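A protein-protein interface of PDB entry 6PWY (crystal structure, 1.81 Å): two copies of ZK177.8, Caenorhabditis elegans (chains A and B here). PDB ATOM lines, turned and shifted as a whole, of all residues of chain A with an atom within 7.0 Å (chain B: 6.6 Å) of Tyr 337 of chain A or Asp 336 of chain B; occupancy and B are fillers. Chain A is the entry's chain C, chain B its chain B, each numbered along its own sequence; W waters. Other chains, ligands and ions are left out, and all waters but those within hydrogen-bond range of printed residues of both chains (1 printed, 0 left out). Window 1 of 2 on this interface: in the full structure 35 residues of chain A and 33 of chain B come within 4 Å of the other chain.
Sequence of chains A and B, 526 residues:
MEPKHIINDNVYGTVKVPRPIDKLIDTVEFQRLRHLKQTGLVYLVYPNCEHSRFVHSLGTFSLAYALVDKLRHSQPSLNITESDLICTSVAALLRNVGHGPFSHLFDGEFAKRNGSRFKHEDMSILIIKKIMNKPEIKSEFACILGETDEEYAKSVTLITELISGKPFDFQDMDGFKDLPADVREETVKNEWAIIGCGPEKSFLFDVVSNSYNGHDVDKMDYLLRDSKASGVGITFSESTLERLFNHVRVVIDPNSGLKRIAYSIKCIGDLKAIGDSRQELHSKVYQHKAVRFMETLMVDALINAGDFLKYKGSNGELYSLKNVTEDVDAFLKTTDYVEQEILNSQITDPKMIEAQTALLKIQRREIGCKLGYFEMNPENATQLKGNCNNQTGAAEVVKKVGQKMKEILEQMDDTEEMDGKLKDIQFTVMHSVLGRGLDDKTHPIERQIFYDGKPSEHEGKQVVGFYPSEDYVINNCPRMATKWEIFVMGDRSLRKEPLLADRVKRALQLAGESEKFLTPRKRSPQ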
ATOM      1  N   ARG A  34      18.738  13.016 -13.526  1.00  0.00           N
ATOM      2  CA  ARG A  34      17.882  12.502 -12.435  1.00  0.00           C
ATOM      3  C   ARG A  34      18.470  11.211 -11.834  1.00  0.00           C
ATOM      4  O   ARG A  34      18.100  10.882 -10.694  1.00  0.00           O
ATOM      5  CB  ARG A  34      16.488  12.237 -12.997  1.00  0.00           C
ATOM      6  CG  ARG A  34      15.731  13.530 -13.248  1.00  0.00           C
ATOM      7  CD  ARG A  34      14.322  13.188 -13.585  1.00  0.00           C
ATOM      8  NE  ARG A  34      13.455  14.299 -14.022  1.00  0.00           N
ATOM      9  CZ  ARG A  34      12.637  14.995 -13.275  1.00  0.00           C
ATOM     10  NH1 ARG A  34      12.629  14.890 -11.969  1.00  0.00           N
ATOM     11  NH2 ARG A  34      11.802  15.810 -13.867  1.00  0.00           N
ATOM     12  N   HIS A  35      19.307  10.500 -12.599  1.00  0.00           N
ATOM     13  CA  HIS A  35      19.768   9.130 -12.260  1.00  0.00           C
ATOM     14  C   HIS A  35      21.250   9.156 -11.885  1.00  0.00           C
ATOM     15  O   HIS A  35      21.888   8.084 -11.961  1.00  0.00           O
ATOM     16  CB  HIS A  35      19.486   8.209 -13.407  1.00  0.00           C
ATOM     17  CG  HIS A  35      18.050   8.288 -13.834  1.00  0.00           C
ATOM     18  ND1 HIS A  35      17.011   8.048 -12.972  1.00  0.00           N
ATOM     19  CD2 HIS A  35      17.492   8.618 -15.016  1.00  0.00           C
ATOM     20  CE1 HIS A  35      15.855   8.239 -13.596  1.00  0.00           C
ATOM     21  NE2 HIS A  35      16.141   8.572 -14.860  1.00  0.00           N
ATOM     22  N   LEU A  36      21.789  10.349 -11.585  1.00  0.00           N
ATOM     23  CA  LEU A  36      23.137  10.538 -11.024  1.00  0.00           C
ATOM     24  C   LEU A  36      22.984  11.237  -9.666  1.00  0.00           C
ATOM     25  O   LEU A  36      22.503  12.334  -9.629  1.00  0.00           O
ATOM     26  CB  LEU A  36      23.991  11.371 -11.986  1.00  0.00           C
ATOM     27  CG  LEU A  36      24.192  10.808 -13.364  1.00  0.00           C
ATOM     28  CD1 LEU A  36      24.933  11.810 -14.206  1.00  0.00           C
ATOM     29  CD2 LEU A  36      24.953   9.474 -13.366  1.00  0.00           C
ATOM     30  N   LYS A  37      23.420  10.600  -8.577  1.00  0.00           N
ATOM     31  CA  LYS A  37      23.450  11.240  -7.262  1.00  0.00           C
ATOM     32  C   LYS A  37      24.518  12.332  -7.265  1.00  0.00           C
ATOM     33  O   LYS A  37      25.666  12.048  -7.644  1.00  0.00           O
ATOM     34  CB  LYS A  37      23.666  10.213  -6.155  1.00  0.00           C
ATOM     35  CG  LYS A  37      22.385   9.498  -5.717  1.00  0.00           C
ATOM     36  CD  LYS A  37      22.590   8.410  -4.695  1.00  0.00           C
ATOM     37  CE  LYS A  37      23.291   7.214  -5.292  1.00  0.00           C
ATOM     38  NZ  LYS A  37      22.448   6.443  -6.226  1.00  0.00           N
ATOM     39  N   PRO A 101      28.670   8.031 -14.016  1.00  0.00           N
ATOM     40  CA  PRO A 101      28.218   7.441 -12.763  1.00  0.00           C
ATOM     41  C   PRO A 101      29.250   7.641 -11.645  1.00  0.00           C
ATOM     42  O   PRO A 101      30.421   7.526 -11.914  1.00  0.00           O
ATOM     43  CB  PRO A 101      28.139   5.935 -13.097  1.00  0.00           C
ATOM     44  CG  PRO A 101      28.282   5.796 -14.546  1.00  0.00           C
ATOM     45  CD  PRO A 101      28.966   7.049 -15.047  1.00  0.00           C
ATOM     46  N   PHE A 102      28.801   7.910 -10.427  1.00  0.00           N
ATOM     47  CA  PHE A 102      29.705   8.073  -9.265  1.00  0.00           C
ATOM     48  C   PHE A 102      30.921   8.923  -9.697  1.00  0.00           C
ATOM     49  O   PHE A 102      32.083   8.475  -9.517  1.00  0.00           O
ATOM     50  CB  PHE A 102      30.118   6.672  -8.761  1.00  0.00           C
ATOM     51  CG  PHE A 102      28.950   5.809  -8.388  1.00  0.00           C
ATOM     52  CD1 PHE A 102      28.136   6.192  -7.344  1.00  0.00           C
ATOM     53  CD2 PHE A 102      28.621   4.701  -9.130  1.00  0.00           C
ATOM     54  CE1 PHE A 102      26.996   5.457  -7.026  1.00  0.00           C
ATOM     55  CE2 PHE A 102      27.517   3.941  -8.778  1.00  0.00           C
ATOM     56  CZ  PHE A 102      26.712   4.319  -7.739  1.00  0.00           C
ATOM     57  N   TYR A 311      27.886  -0.502 -23.851  1.00  0.00           N
ATOM     58  CA  TYR A 311      26.908   0.562 -24.163  1.00  0.00           C
ATOM     59  C   TYR A 311      27.002   0.905 -25.656  1.00  0.00           C
ATOM     60  O   TYR A 311      28.100   1.096 -26.174  1.00  0.00           O
ATOM     61  CB  TYR A 311      27.237   1.783 -23.298  1.00  0.00           C
ATOM     62  CG  TYR A 311      27.271   1.441 -21.832  1.00  0.00           C
ATOM     63  CD1 TYR A 311      26.085   1.381 -21.097  1.00  0.00           C
ATOM     64  CD2 TYR A 311      28.451   1.089 -21.217  1.00  0.00           C
ATOM     65  CE1 TYR A 311      26.100   1.016 -19.764  1.00  0.00           C
ATOM     66  CE2 TYR A 311      28.472   0.744 -19.868  1.00  0.00           C
ATOM     67  CZ  TYR A 311      27.308   0.746 -19.139  1.00  0.00           C
ATOM     68  OH  TYR A 311      27.338   0.355 -17.835  1.00  0.00           O
ATOM     69  N   THR A 334      25.103   5.709 -19.620  1.00  0.00           N
ATOM     70  CA  THR A 334      25.601   5.358 -18.273  1.00  0.00           C
ATOM     71  C   THR A 334      24.826   6.138 -17.207  1.00  0.00           C
ATOM     72  O   THR A 334      24.561   7.329 -17.381  1.00  0.00           O
ATOM     73  CB  THR A 334      27.127   5.531 -18.128  1.00  0.00           C
ATOM     74  OG1 THR A 334      27.444   6.923 -18.213  1.00  0.00           O
ATOM     75  CG2 THR A 334      27.885   4.724 -19.147  1.00  0.00           C
ATOM     76  N   THR A 335      24.523   5.478 -16.100  1.00  0.00           N
ATOM     77  CA  THR A 335      23.965   6.115 -14.880  1.00  0.00           C
ATOM     78  C   THR A 335      24.489   5.369 -13.660  1.00  0.00           C
ATOM     79  O   THR A 335      25.223   4.406 -13.819  1.00  0.00           O
ATOM     80  CB  THR A 335      22.425   6.180 -14.889  1.00  0.00           C
ATOM     81  OG1 THR A 335      21.944   4.863 -14.746  1.00  0.00           O
ATOM     82  CG2 THR A 335      21.792   6.743 -16.160  1.00  0.00           C
ATOM     83  N   ASP A 336      24.018   5.768 -12.477  1.00  0.00           N
ATOM     84  CA  ASP A 336      24.346   5.100 -11.200  1.00  0.00           C
ATOM     85  C   ASP A 336      23.746   3.667 -11.221  1.00  0.00           C
ATOM     86  O   ASP A 336      24.143   2.865 -10.391  1.00  0.00           O
ATOM     87  CB  ASP A 336      23.822   5.911 -10.000  1.00  0.00           C
ATOM     88  CG  ASP A 336      24.544   7.220  -9.691  1.00  0.00           C
ATOM     89  OD1 ASP A 336      25.605   7.516 -10.300  1.00  0.00           O
ATOM     90  OD2 ASP A 336      24.024   7.939  -8.743  1.00  0.00           O
ATOM     91  N   TYR A 337      22.867   3.353 -12.163  1.00  0.00           N
ATOM     92  CA  TYR A 337      22.360   1.967 -12.275  1.00  0.00           C
ATOM     93  C   TYR A 337      23.466   1.001 -12.760  1.00  0.00           C
ATOM     94  O   TYR A 337      23.260  -0.196 -12.629  1.00  0.00           O
ATOM     95  CB  TYR A 337      21.015   1.969 -12.971  1.00  0.00           C
ATOM     96  CG  TYR A 337      19.938   2.669 -12.178  1.00  0.00           C
ATOM     97  CD1 TYR A 337      19.419   2.107 -11.029  1.00  0.00           C
ATOM     98  CD2 TYR A 337      19.390   3.867 -12.604  1.00  0.00           C
ATOM     99  CE1 TYR A 337      18.446   2.748 -10.287  1.00  0.00           C
ATOM    100  CE2 TYR A 337      18.421   4.529 -11.859  1.00  0.00           C
ATOM    101  CZ  TYR A 337      17.911   3.947 -10.716  1.00  0.00           C
ATOM    102  OH  TYR A 337      16.868   4.529 -10.035  1.00  0.00           O
ATOM    103  N   VAL A 338      24.661   1.485 -13.109  1.00  0.00           N
ATOM    104  CA  VAL A 338      25.833   0.591 -13.337  1.00  0.00           C
ATOM    105  C   VAL A 338      25.984  -0.401 -12.154  1.00  0.00           C
ATOM    106  O   VAL A 338      26.343  -1.557 -12.383  1.00  0.00           O
ATOM    107  CB  VAL A 338      27.132   1.389 -13.627  1.00  0.00           C
ATOM    108  CG1 VAL A 338      27.642   2.134 -12.429  1.00  0.00           C
ATOM    109  CG2 VAL A 338      28.218   0.452 -14.103  1.00  0.00           C
ATOM    110  N   GLU A 339      25.766   0.026 -10.910  1.00  0.00           N
ATOM    111  CA  GLU A 339      25.856  -0.849  -9.724  1.00  0.00           C
ATOM    112  C   GLU A 339      24.884  -2.045  -9.890  1.00  0.00           C
ATOM    113  O   GLU A 339      25.291  -3.223  -9.710  1.00  0.00           O
ATOM    114  CB  GLU A 339      25.481  -0.058  -8.478  1.00  0.00           C
ATOM    115  CG  GLU A 339      25.668  -0.848  -7.210  1.00  0.00           C
ATOM    116  CD  GLU A 339      24.980  -0.272  -5.982  1.00  0.00           C
ATOM    117  OE1 GLU A 339      24.511   0.954  -6.066  1.00  0.00           O
ATOM    118  OE2 GLU A 339      24.868  -1.070  -4.941  1.00  0.00           O
ATOM    119  N   GLN A 340      23.652  -1.781 -10.307  1.00  0.00           N
ATOM    120  CA  GLN A 340      22.649  -2.863 -10.476  1.00  0.00           C
ATOM    121  C   GLN A 340      23.004  -3.741 -11.693  1.00  0.00           C
ATOM    122  O   GLN A 340      22.766  -4.948 -11.638  1.00  0.00           O
ATOM    123  CB  GLN A 340      21.246  -2.243 -10.476  1.00  0.00           C
ATOM    124  CG  GLN A 340      20.201  -3.248 -10.088  1.00  0.00           C
ATOM    125  CD  GLN A 340      20.228  -3.658  -8.645  1.00  0.00           C
ATOM    126  OE1 GLN A 340      20.392  -2.793  -7.755  1.00  0.00           O
ATOM    127  NE2 GLN A 340      20.144  -4.987  -8.428  1.00  0.00           N
ATOM    128  N   GLU A 341      23.546  -3.166 -12.752  1.00  0.00           N
ATOM    129  CA  GLU A 341      24.039  -3.912 -13.938  1.00  0.00           C
ATOM    130  C   GLU A 341      25.061  -4.970 -13.503  1.00  0.00           C
ATOM    131  O   GLU A 341      24.969  -6.100 -13.925  1.00  0.00           O
ATOM    132  CB  GLU A 341      24.777  -3.008 -14.929  1.00  0.00           C
ATOM    133  CG  GLU A 341      23.879  -2.147 -15.765  1.00  0.00           C
ATOM    134  CD  GLU A 341      24.624  -1.385 -16.863  1.00  0.00           C
ATOM    135  OE1 GLU A 341      24.915  -0.177 -16.649  1.00  0.00           O
ATOM    136  OE2 GLU A 341      24.946  -2.001 -17.885  1.00  0.00           O
ATOM    137  N   ILE A 342      26.001  -4.596 -12.641  1.00  0.00           N
ATOM    138  CA  ILE A 342      26.996  -5.549 -12.076  1.00  0.00           C
ATOM    139  C   ILE A 342      26.247  -6.609 -11.259  1.00  0.00           C
ATOM    140  O   ILE A 342      26.459  -7.827 -11.520  1.00  0.00           O
ATOM    141  CB  ILE A 342      28.090  -4.825 -11.281  1.00  0.00           C
ATOM    142  CG1 ILE A 342      28.835  -3.873 -12.239  1.00  0.00           C
ATOM    143  CG2 ILE A 342      29.008  -5.848 -10.613  1.00  0.00           C
ATOM    144  CD1 ILE A 342      29.789  -2.918 -11.566  1.00  0.00           C
ATOM    145  N   LEU A 343      25.463  -6.186 -10.275  1.00  0.00           N
ATOM    146  CA  LEU A 343      24.767  -7.129  -9.351  1.00  0.00           C
ATOM    147  C   LEU A 343      23.938  -8.157 -10.148  1.00  0.00           C
ATOM    148  O   LEU A 343      23.917  -9.287  -9.703  1.00  0.00           O
ATOM    149  CB  LEU A 343      23.886  -6.347  -8.375  1.00  0.00           C
ATOM    150  CG  LEU A 343      24.632  -5.658  -7.229  1.00  0.00           C
ATOM    151  CD1 LEU A 343      23.688  -4.722  -6.459  1.00  0.00           C
ATOM    152  CD2 LEU A 343      25.272  -6.688  -6.308  1.00  0.00           C
ATOM    153  N   HIS B  35      16.858   1.866  -3.782  1.00  0.00           N
ATOM    154  CA  HIS B  35      16.752   1.961  -5.273  1.00  0.00           C
ATOM    155  C   HIS B  35      15.288   1.880  -5.686  1.00  0.00           C
ATOM    156  O   HIS B  35      15.052   1.564  -6.864  1.00  0.00           O
ATOM    157  CB  HIS B  35      17.589   0.875  -5.891  1.00  0.00           C
ATOM    158  CG  HIS B  35      18.999   0.922  -5.383  1.00  0.00           C
ATOM    159  ND1 HIS B  35      19.794   2.063  -5.462  1.00  0.00           N
ATOM    160  CD2 HIS B  35      19.747  -0.005  -4.740  1.00  0.00           C
ATOM    161  CE1 HIS B  35      20.972   1.842  -4.875  1.00  0.00           C
ATOM    162  NE2 HIS B  35      20.954   0.545  -4.449  1.00  0.00           N
ATOM    163  N   LEU B  36      14.355   2.099  -4.745  1.00  0.00           N
ATOM    164  CA  LEU B  36      12.903   2.242  -5.001  1.00  0.00           C
ATOM    165  C   LEU B  36      12.455   3.604  -4.490  1.00  0.00           C
ATOM    166  O   LEU B  36      12.548   3.834  -3.318  1.00  0.00           O
ATOM    167  CB  LEU B  36      12.122   1.109  -4.322  1.00  0.00           C
ATOM    168  CG  LEU B  36      12.488  -0.306  -4.719  1.00  0.00           C
ATOM    169  CD1 LEU B  36      11.700  -1.278  -3.864  1.00  0.00           C
ATOM    170  CD2 LEU B  36      12.183  -0.593  -6.170  1.00  0.00           C
ATOM    171  N   LYS B  37      11.973   4.470  -5.370  1.00  0.00           N
ATOM    172  CA  LYS B  37      11.398   5.757  -4.965  1.00  0.00           C
ATOM    173  C   LYS B  37      10.090   5.497  -4.208  1.00  0.00           C
ATOM    174  O   LYS B  37       9.229   4.772  -4.728  1.00  0.00           O
ATOM    175  CB  LYS B  37      11.200   6.684  -6.150  1.00  0.00           C
ATOM    176  CG  LYS B  37      12.463   7.427  -6.560  1.00  0.00           C
ATOM    177  CD  LYS B  37      12.321   8.257  -7.824  1.00  0.00           C
ATOM    178  CE  LYS B  37      12.252   7.377  -9.052  1.00  0.00           C
ATOM    179  NZ  LYS B  37      13.567   6.766  -9.372  1.00  0.00           N
ATOM    180  N   GLN B  38       9.990   6.072  -3.017  1.00  0.00           N
ATOM    181  CA  GLN B  38       8.805   6.017  -2.165  1.00  0.00           C
ATOM    182  C   GLN B  38       7.585   6.509  -2.921  1.00  0.00           C
ATOM    183  O   GLN B  38       6.527   5.922  -2.675  1.00  0.00           O
ATOM    184  CB  GLN B  38       9.025   6.904  -0.934  1.00  0.00           C
ATOM    185  CG  GLN B  38       7.855   6.953   0.028  1.00  0.00           C
ATOM    186  CD  GLN B  38       7.552   5.666   0.739  1.00  0.00           C
ATOM    187  OE1 GLN B  38       8.426   4.818   0.879  1.00  0.00           O
ATOM    188  NE2 GLN B  38       6.318   5.552   1.258  1.00  0.00           N
ATOM    189  N   GLY B  40       7.168   6.804  -6.419  1.00  0.00           N
ATOM    190  CA  GLY B  40       7.078   6.385  -7.838  1.00  0.00           C
ATOM    191  C   GLY B  40       7.531   7.469  -8.817  1.00  0.00           C
ATOM    192  O   GLY B  40       8.621   8.059  -8.640  1.00  0.00           O
ATOM    193  N   ARG B  53      12.390   4.264  -0.451  1.00  0.00           N
ATOM    194  CA  ARG B  53      11.662   3.430   0.509  1.00  0.00           C
ATOM    195  C   ARG B  53      12.528   3.155   1.746  1.00  0.00           C
ATOM    196  O   ARG B  53      11.994   2.955   2.841  1.00  0.00           O
ATOM    197  CB  ARG B  53      11.134   2.158  -0.180  1.00  0.00           C
ATOM    198  CG  ARG B  53      10.042   2.439  -1.192  1.00  0.00           C
ATOM    199  CD  ARG B  53       9.371   1.172  -1.719  1.00  0.00           C
ATOM    200  NE  ARG B  53       8.453   1.534  -2.790  1.00  0.00           N
ATOM    201  CZ  ARG B  53       7.276   2.109  -2.641  1.00  0.00           C
ATOM    202  NH1 ARG B  53       6.770   2.374  -1.455  1.00  0.00           N
ATOM    203  NH2 ARG B  53       6.588   2.444  -3.724  1.00  0.00           N
ATOM    204  N   GLY B 100       7.659  -3.791  -5.503  1.00  0.00           N
ATOM    205  CA  GLY B 100       8.322  -3.846  -6.804  1.00  0.00           C
ATOM    206  C   GLY B 100       8.755  -2.475  -7.265  1.00  0.00           C
ATOM    207  O   GLY B 100       8.445  -1.474  -6.650  1.00  0.00           O
ATOM    208  N   PRO B 101       9.382  -2.379  -8.453  1.00  0.00           N
ATOM    209  CA  PRO B 101       9.656  -1.088  -9.066  1.00  0.00           C
ATOM    210  C   PRO B 101       8.364  -0.305  -9.319  1.00  0.00           C
ATOM    211  O   PRO B 101       7.364  -0.935  -9.721  1.00  0.00           O
ATOM    212  CB  PRO B 101      10.245  -1.484 -10.426  1.00  0.00           C
ATOM    213  CG  PRO B 101      10.549  -2.919 -10.381  1.00  0.00           C
ATOM    214  CD  PRO B 101       9.666  -3.513  -9.327  1.00  0.00           C
ATOM    215  N   PHE B 102       8.358   0.994  -9.111  1.00  0.00           N
ATOM    216  CA  PHE B 102       7.176   1.856  -9.383  1.00  0.00           C
ATOM    217  C   PHE B 102       5.928   1.133  -8.836  1.00  0.00           C
ATOM    218  O   PHE B 102       4.954   0.872  -9.623  1.00  0.00           O
ATOM    219  CB  PHE B 102       7.077   2.111 -10.912  1.00  0.00           C
ATOM    220  CG  PHE B 102       8.302   2.759 -11.475  1.00  0.00           C
ATOM    221  CD1 PHE B 102       8.633   4.027 -11.064  1.00  0.00           C
ATOM    222  CD2 PHE B 102       9.156   2.087 -12.317  1.00  0.00           C
ATOM    223  CE1 PHE B 102       9.816   4.646 -11.492  1.00  0.00           C
ATOM    224  CE2 PHE B 102      10.298   2.715 -12.796  1.00  0.00           C
ATOM    225  CZ  PHE B 102      10.647   3.980 -12.353  1.00  0.00           C
ATOM    226  N   SER B 103       5.953   0.822  -7.542  1.00  0.00           N
ATOM    227  CA  SER B 103       5.008  -0.113  -6.874  1.00  0.00           C
ATOM    228  C   SER B 103       3.549   0.106  -7.297  1.00  0.00           C
ATOM    229  O   SER B 103       2.855  -0.905  -7.562  1.00  0.00           O
ATOM    230  CB  SER B 103       5.124  -0.043  -5.362  1.00  0.00           C
ATOM    231  OG  SER B 103       4.236  -0.956  -4.739  1.00  0.00           O
ATOM    232  N   THR B 334      14.851  -6.828  -8.898  1.00  0.00           N
ATOM    233  CA  THR B 334      14.125  -5.718  -9.554  1.00  0.00           C
ATOM    234  C   THR B 334      14.317  -4.424  -8.765  1.00  0.00           C
ATOM    235  O   THR B 334      14.279  -4.447  -7.508  1.00  0.00           O
ATOM    236  CB  THR B 334      12.637  -6.023  -9.805  1.00  0.00           C
ATOM    237  OG1 THR B 334      11.951  -6.102  -8.542  1.00  0.00           O
ATOM    238  CG2 THR B 334      12.458  -7.268 -10.625  1.00  0.00           C
ATOM    239  N   THR B 335      14.500  -3.316  -9.476  1.00  0.00           N
ATOM    240  CA  THR B 335      14.513  -1.944  -8.893  1.00  0.00           C
ATOM    241  C   THR B 335      13.914  -0.977  -9.907  1.00  0.00           C
ATOM    242  O   THR B 335      13.555  -1.408 -10.996  1.00  0.00           O
ATOM    243  CB  THR B 335      15.902  -1.504  -8.429  1.00  0.00           C
ATOM    244  OG1 THR B 335      16.682  -1.296  -9.582  1.00  0.00           O
ATOM    245  CG2 THR B 335      16.635  -2.485  -7.517  1.00  0.00           C
ATOM    246  N   ASP B 336      13.904   0.308  -9.565  1.00  0.00           N
ATOM    247  CA  ASP B 336      13.502   1.402 -10.465  1.00  0.00           C
ATOM    248  C   ASP B 336      14.463   1.462 -11.673  1.00  0.00           C
ATOM    249  O   ASP B 336      14.113   2.086 -12.655  1.00  0.00           O
ATOM    250  CB  ASP B 336      13.442   2.743  -9.708  1.00  0.00           C
ATOM    251  CG  ASP B 336      12.267   2.915  -8.734  1.00  0.00           C
ATOM    252  OD1 ASP B 336      11.370   2.058  -8.662  1.00  0.00           O
ATOM    253  OD2 ASP B 336      12.266   3.991  -8.055  1.00  0.00           O
ATOM    254  N   TYR B 337      15.604   0.815 -11.609  1.00  0.00           N
ATOM    255  CA  TYR B 337      16.605   0.515 -12.676  1.00  0.00           C
ATOM    256  C   TYR B 337      15.915  -0.063 -13.920  1.00  0.00           C
ATOM    257  O   TYR B 337      16.426   0.049 -15.025  1.00  0.00           O
ATOM    258  CB  TYR B 337      17.596  -0.530 -12.137  1.00  0.00           C
ATOM    259  CG  TYR B 337      18.486  -1.242 -13.133  1.00  0.00           C
ATOM    260  CD1 TYR B 337      19.144  -0.549 -14.137  1.00  0.00           C
ATOM    261  CD2 TYR B 337      18.689  -2.621 -13.078  1.00  0.00           C
ATOM    262  CE1 TYR B 337      19.911  -1.205 -15.088  1.00  0.00           C
ATOM    263  CE2 TYR B 337      19.466  -3.291 -14.014  1.00  0.00           C
ATOM    264  CZ  TYR B 337      20.076  -2.586 -15.033  1.00  0.00           C
ATOM    265  OH  TYR B 337      20.851  -3.222 -15.978  1.00  0.00           O
ATOM    266  N   VAL B 338      14.772  -0.725 -13.732  1.00  0.00           N
ATOM    267  CA  VAL B 338      14.017  -1.353 -14.857  1.00  0.00           C
ATOM    268  C   VAL B 338      13.847  -0.331 -16.013  1.00  0.00           C
ATOM    269  O   VAL B 338      13.928  -0.715 -17.160  1.00  0.00           O
ATOM    270  CB  VAL B 338      12.671  -1.964 -14.381  1.00  0.00           C
ATOM    271  CG1 VAL B 338      11.654  -0.922 -13.990  1.00  0.00           C
ATOM    272  CG2 VAL B 338      12.099  -2.830 -15.466  1.00  0.00           C
ATOM    273  N   GLU B 339      13.608   0.950 -15.715  1.00  0.00           N
ATOM    274  CA  GLU B 339      13.489   2.016 -16.727  1.00  0.00           C
ATOM    275  C   GLU B 339      14.777   2.085 -17.580  1.00  0.00           C
ATOM    276  O   GLU B 339      14.694   2.045 -18.842  1.00  0.00           O
ATOM    277  CB  GLU B 339      13.244   3.349 -16.047  1.00  0.00           C
ATOM    278  CG  GLU B 339      12.958   4.463 -17.031  1.00  0.00           C
ATOM    279  CD  GLU B 339      13.097   5.868 -16.469  1.00  0.00           C
ATOM    280  OE1 GLU B 339      12.945   5.993 -15.211  1.00  0.00           O
ATOM    281  OE2 GLU B 339      13.322   6.847 -17.309  1.00  0.00           O
ATOM    282  N   GLN B 340      15.931   2.063 -16.946  1.00  0.00           N
ATOM    283  CA  GLN B 340      17.228   2.135 -17.684  1.00  0.00           C
ATOM    284  C   GLN B 340      17.478   0.812 -18.447  1.00  0.00           C
ATOM    285  O   GLN B 340      18.034   0.866 -19.536  1.00  0.00           O
ATOM    286  CB  GLN B 340      18.332   2.603 -16.732  1.00  0.00           C
ATOM    287  CG  GLN B 340      19.481   3.216 -17.515  1.00  0.00           C
ATOM    288  CD  GLN B 340      19.214   4.546 -18.143  1.00  0.00           C
ATOM    289  OE1 GLN B 340      18.583   5.418 -17.529  1.00  0.00           O
ATOM    290  NE2 GLN B 340      19.641   4.684 -19.411  1.00  0.00           N
ATOM    291  N   GLU B 341      17.089  -0.336 -17.891  1.00  0.00           N
ATOM    292  CA  GLU B 341      17.177  -1.656 -18.561  1.00  0.00           C
ATOM    293  C   GLU B 341      16.441  -1.601 -19.903  1.00  0.00           C
ATOM    294  O   GLU B 341      16.988  -2.066 -20.888  1.00  0.00           O
ATOM    295  CB  GLU B 341      16.490  -2.774 -17.773  1.00  0.00           C
ATOM    296  CG  GLU B 341      17.256  -3.262 -16.600  1.00  0.00           C
ATOM    297  CD  GLU B 341      16.642  -4.483 -15.898  1.00  0.00           C
ATOM    298  OE1 GLU B 341      15.978  -4.301 -14.868  1.00  0.00           O
ATOM    299  OE2 GLU B 341      16.865  -5.600 -16.364  1.00  0.00           O
HETATM  300  O   HOH W   1      15.558   4.904  -7.533  1.00  0.00           O
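The backbone carbonyl oxygen (O) of His 35 of chain B is in hydrogen-bond range of the backbone NH (N) of Asp 336 of chain B (3.2 Å). The side-chain amino group (NZ) of Lys 37 of chain B is in salt-bridge range of the side-chain carboxylate (OD2) of Asp 336 of chain B (3.3 Å). OD1 of Asp 336 of chain B sits at hydrogen-bond distance from N of Phe 102 of chain B, 3.2 Å away. The side-chain hydroxyl (OG1) of Thr 335 of chain B sits close to the backbone NH (N) of Tyr 337 of chain B (3.1 Å).
Thr 335 of chain A touches Gln 340 of chain B. OH of Tyr 337 of chain A touches CB of Asp 336 of chain B (3.9 Å). CB of Tyr 337 of chain A touches CD1 of Tyr 337 of chain B, 3.3 Å away. Glu 339 of chain A touches His 35 of chain B. CG2 of Thr 335 of chain B touches OE1 of Gln 340 of chain A, at 3.8 Å. Tyr 337 of chain B touches Gln 340 of chain A. CG of Glu 341 of chain A touches OH of Tyr 337 of chain B, 3.2 Å away.
Of the printed residues of chain B, Tyr 337 of chain A touches Asp 336 and Tyr 337. Of the printed residues of chain A, Asp 336 of chain B touches Tyr 337. Of the printed residues of chain B, Gln 340 of chain A touches Thr 335 and Tyr 337. Of the printed residues of chain A, Tyr 337 of chain B touches Tyr 337 (3.3 Å), Gln 340 (3.4 Å) and Glu 341 (3.2 Å). Pro 101 of chain B touches none of the printed residues of chain A. Pro 101 of chain A touches none of the printed residues of chain B. The nearest printed residue of chain B that does not touch Thr 335 of chain A is Tyr 337 of chain B (6.1 Å).
Of the 17 printed residues of chain A, 5 touch a printed residue of chain B. Hydrophobic or aromatic side chains of chain A within 4 Å of the printed part of chain B: Tyr 337. Hydrophobic or aromatic side chains of chain B that line the printed part of chain A: His 35 and Tyr 337. Among the printed residues, 7 pairs touch across the chains.
Thr 335 of chain A touches Gln 340 of chain B, and with the chains exchanged Gln 340 of chain A touches Thr 335 of chain B. Tyr 337 of chain A touches Asp 336 of chain B, but with the chains exchanged Asp 336 of chain A does not touch Tyr 337 of chain B (6.9 Å). Tyr 337 of chain A touches its own counterpart, Tyr 337 of chain B. Gln 340 of chain A touches Tyr 337 of chain B, but with the chains exchanged Tyr 337 of chain A does not touch Gln 340 of chain B (4.4 Å). Positions printed for both chains: 35, 36, 37, 101, 102, 334, 335, 336, 337, 338, 339, 340 and 341.
Water W1 lies within hydrogen-bond range of the side-chain hydroxyl of Tyr 337 of chain A (2.8 Å), the side-chain amino group of Lys 37 of chain B (3.3 Å), the backbone carbonyl oxygen of His 35 of chain B (3.4 Å) and the side-chain carboxylate of Asp 336 of chain B (3.5 Å).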
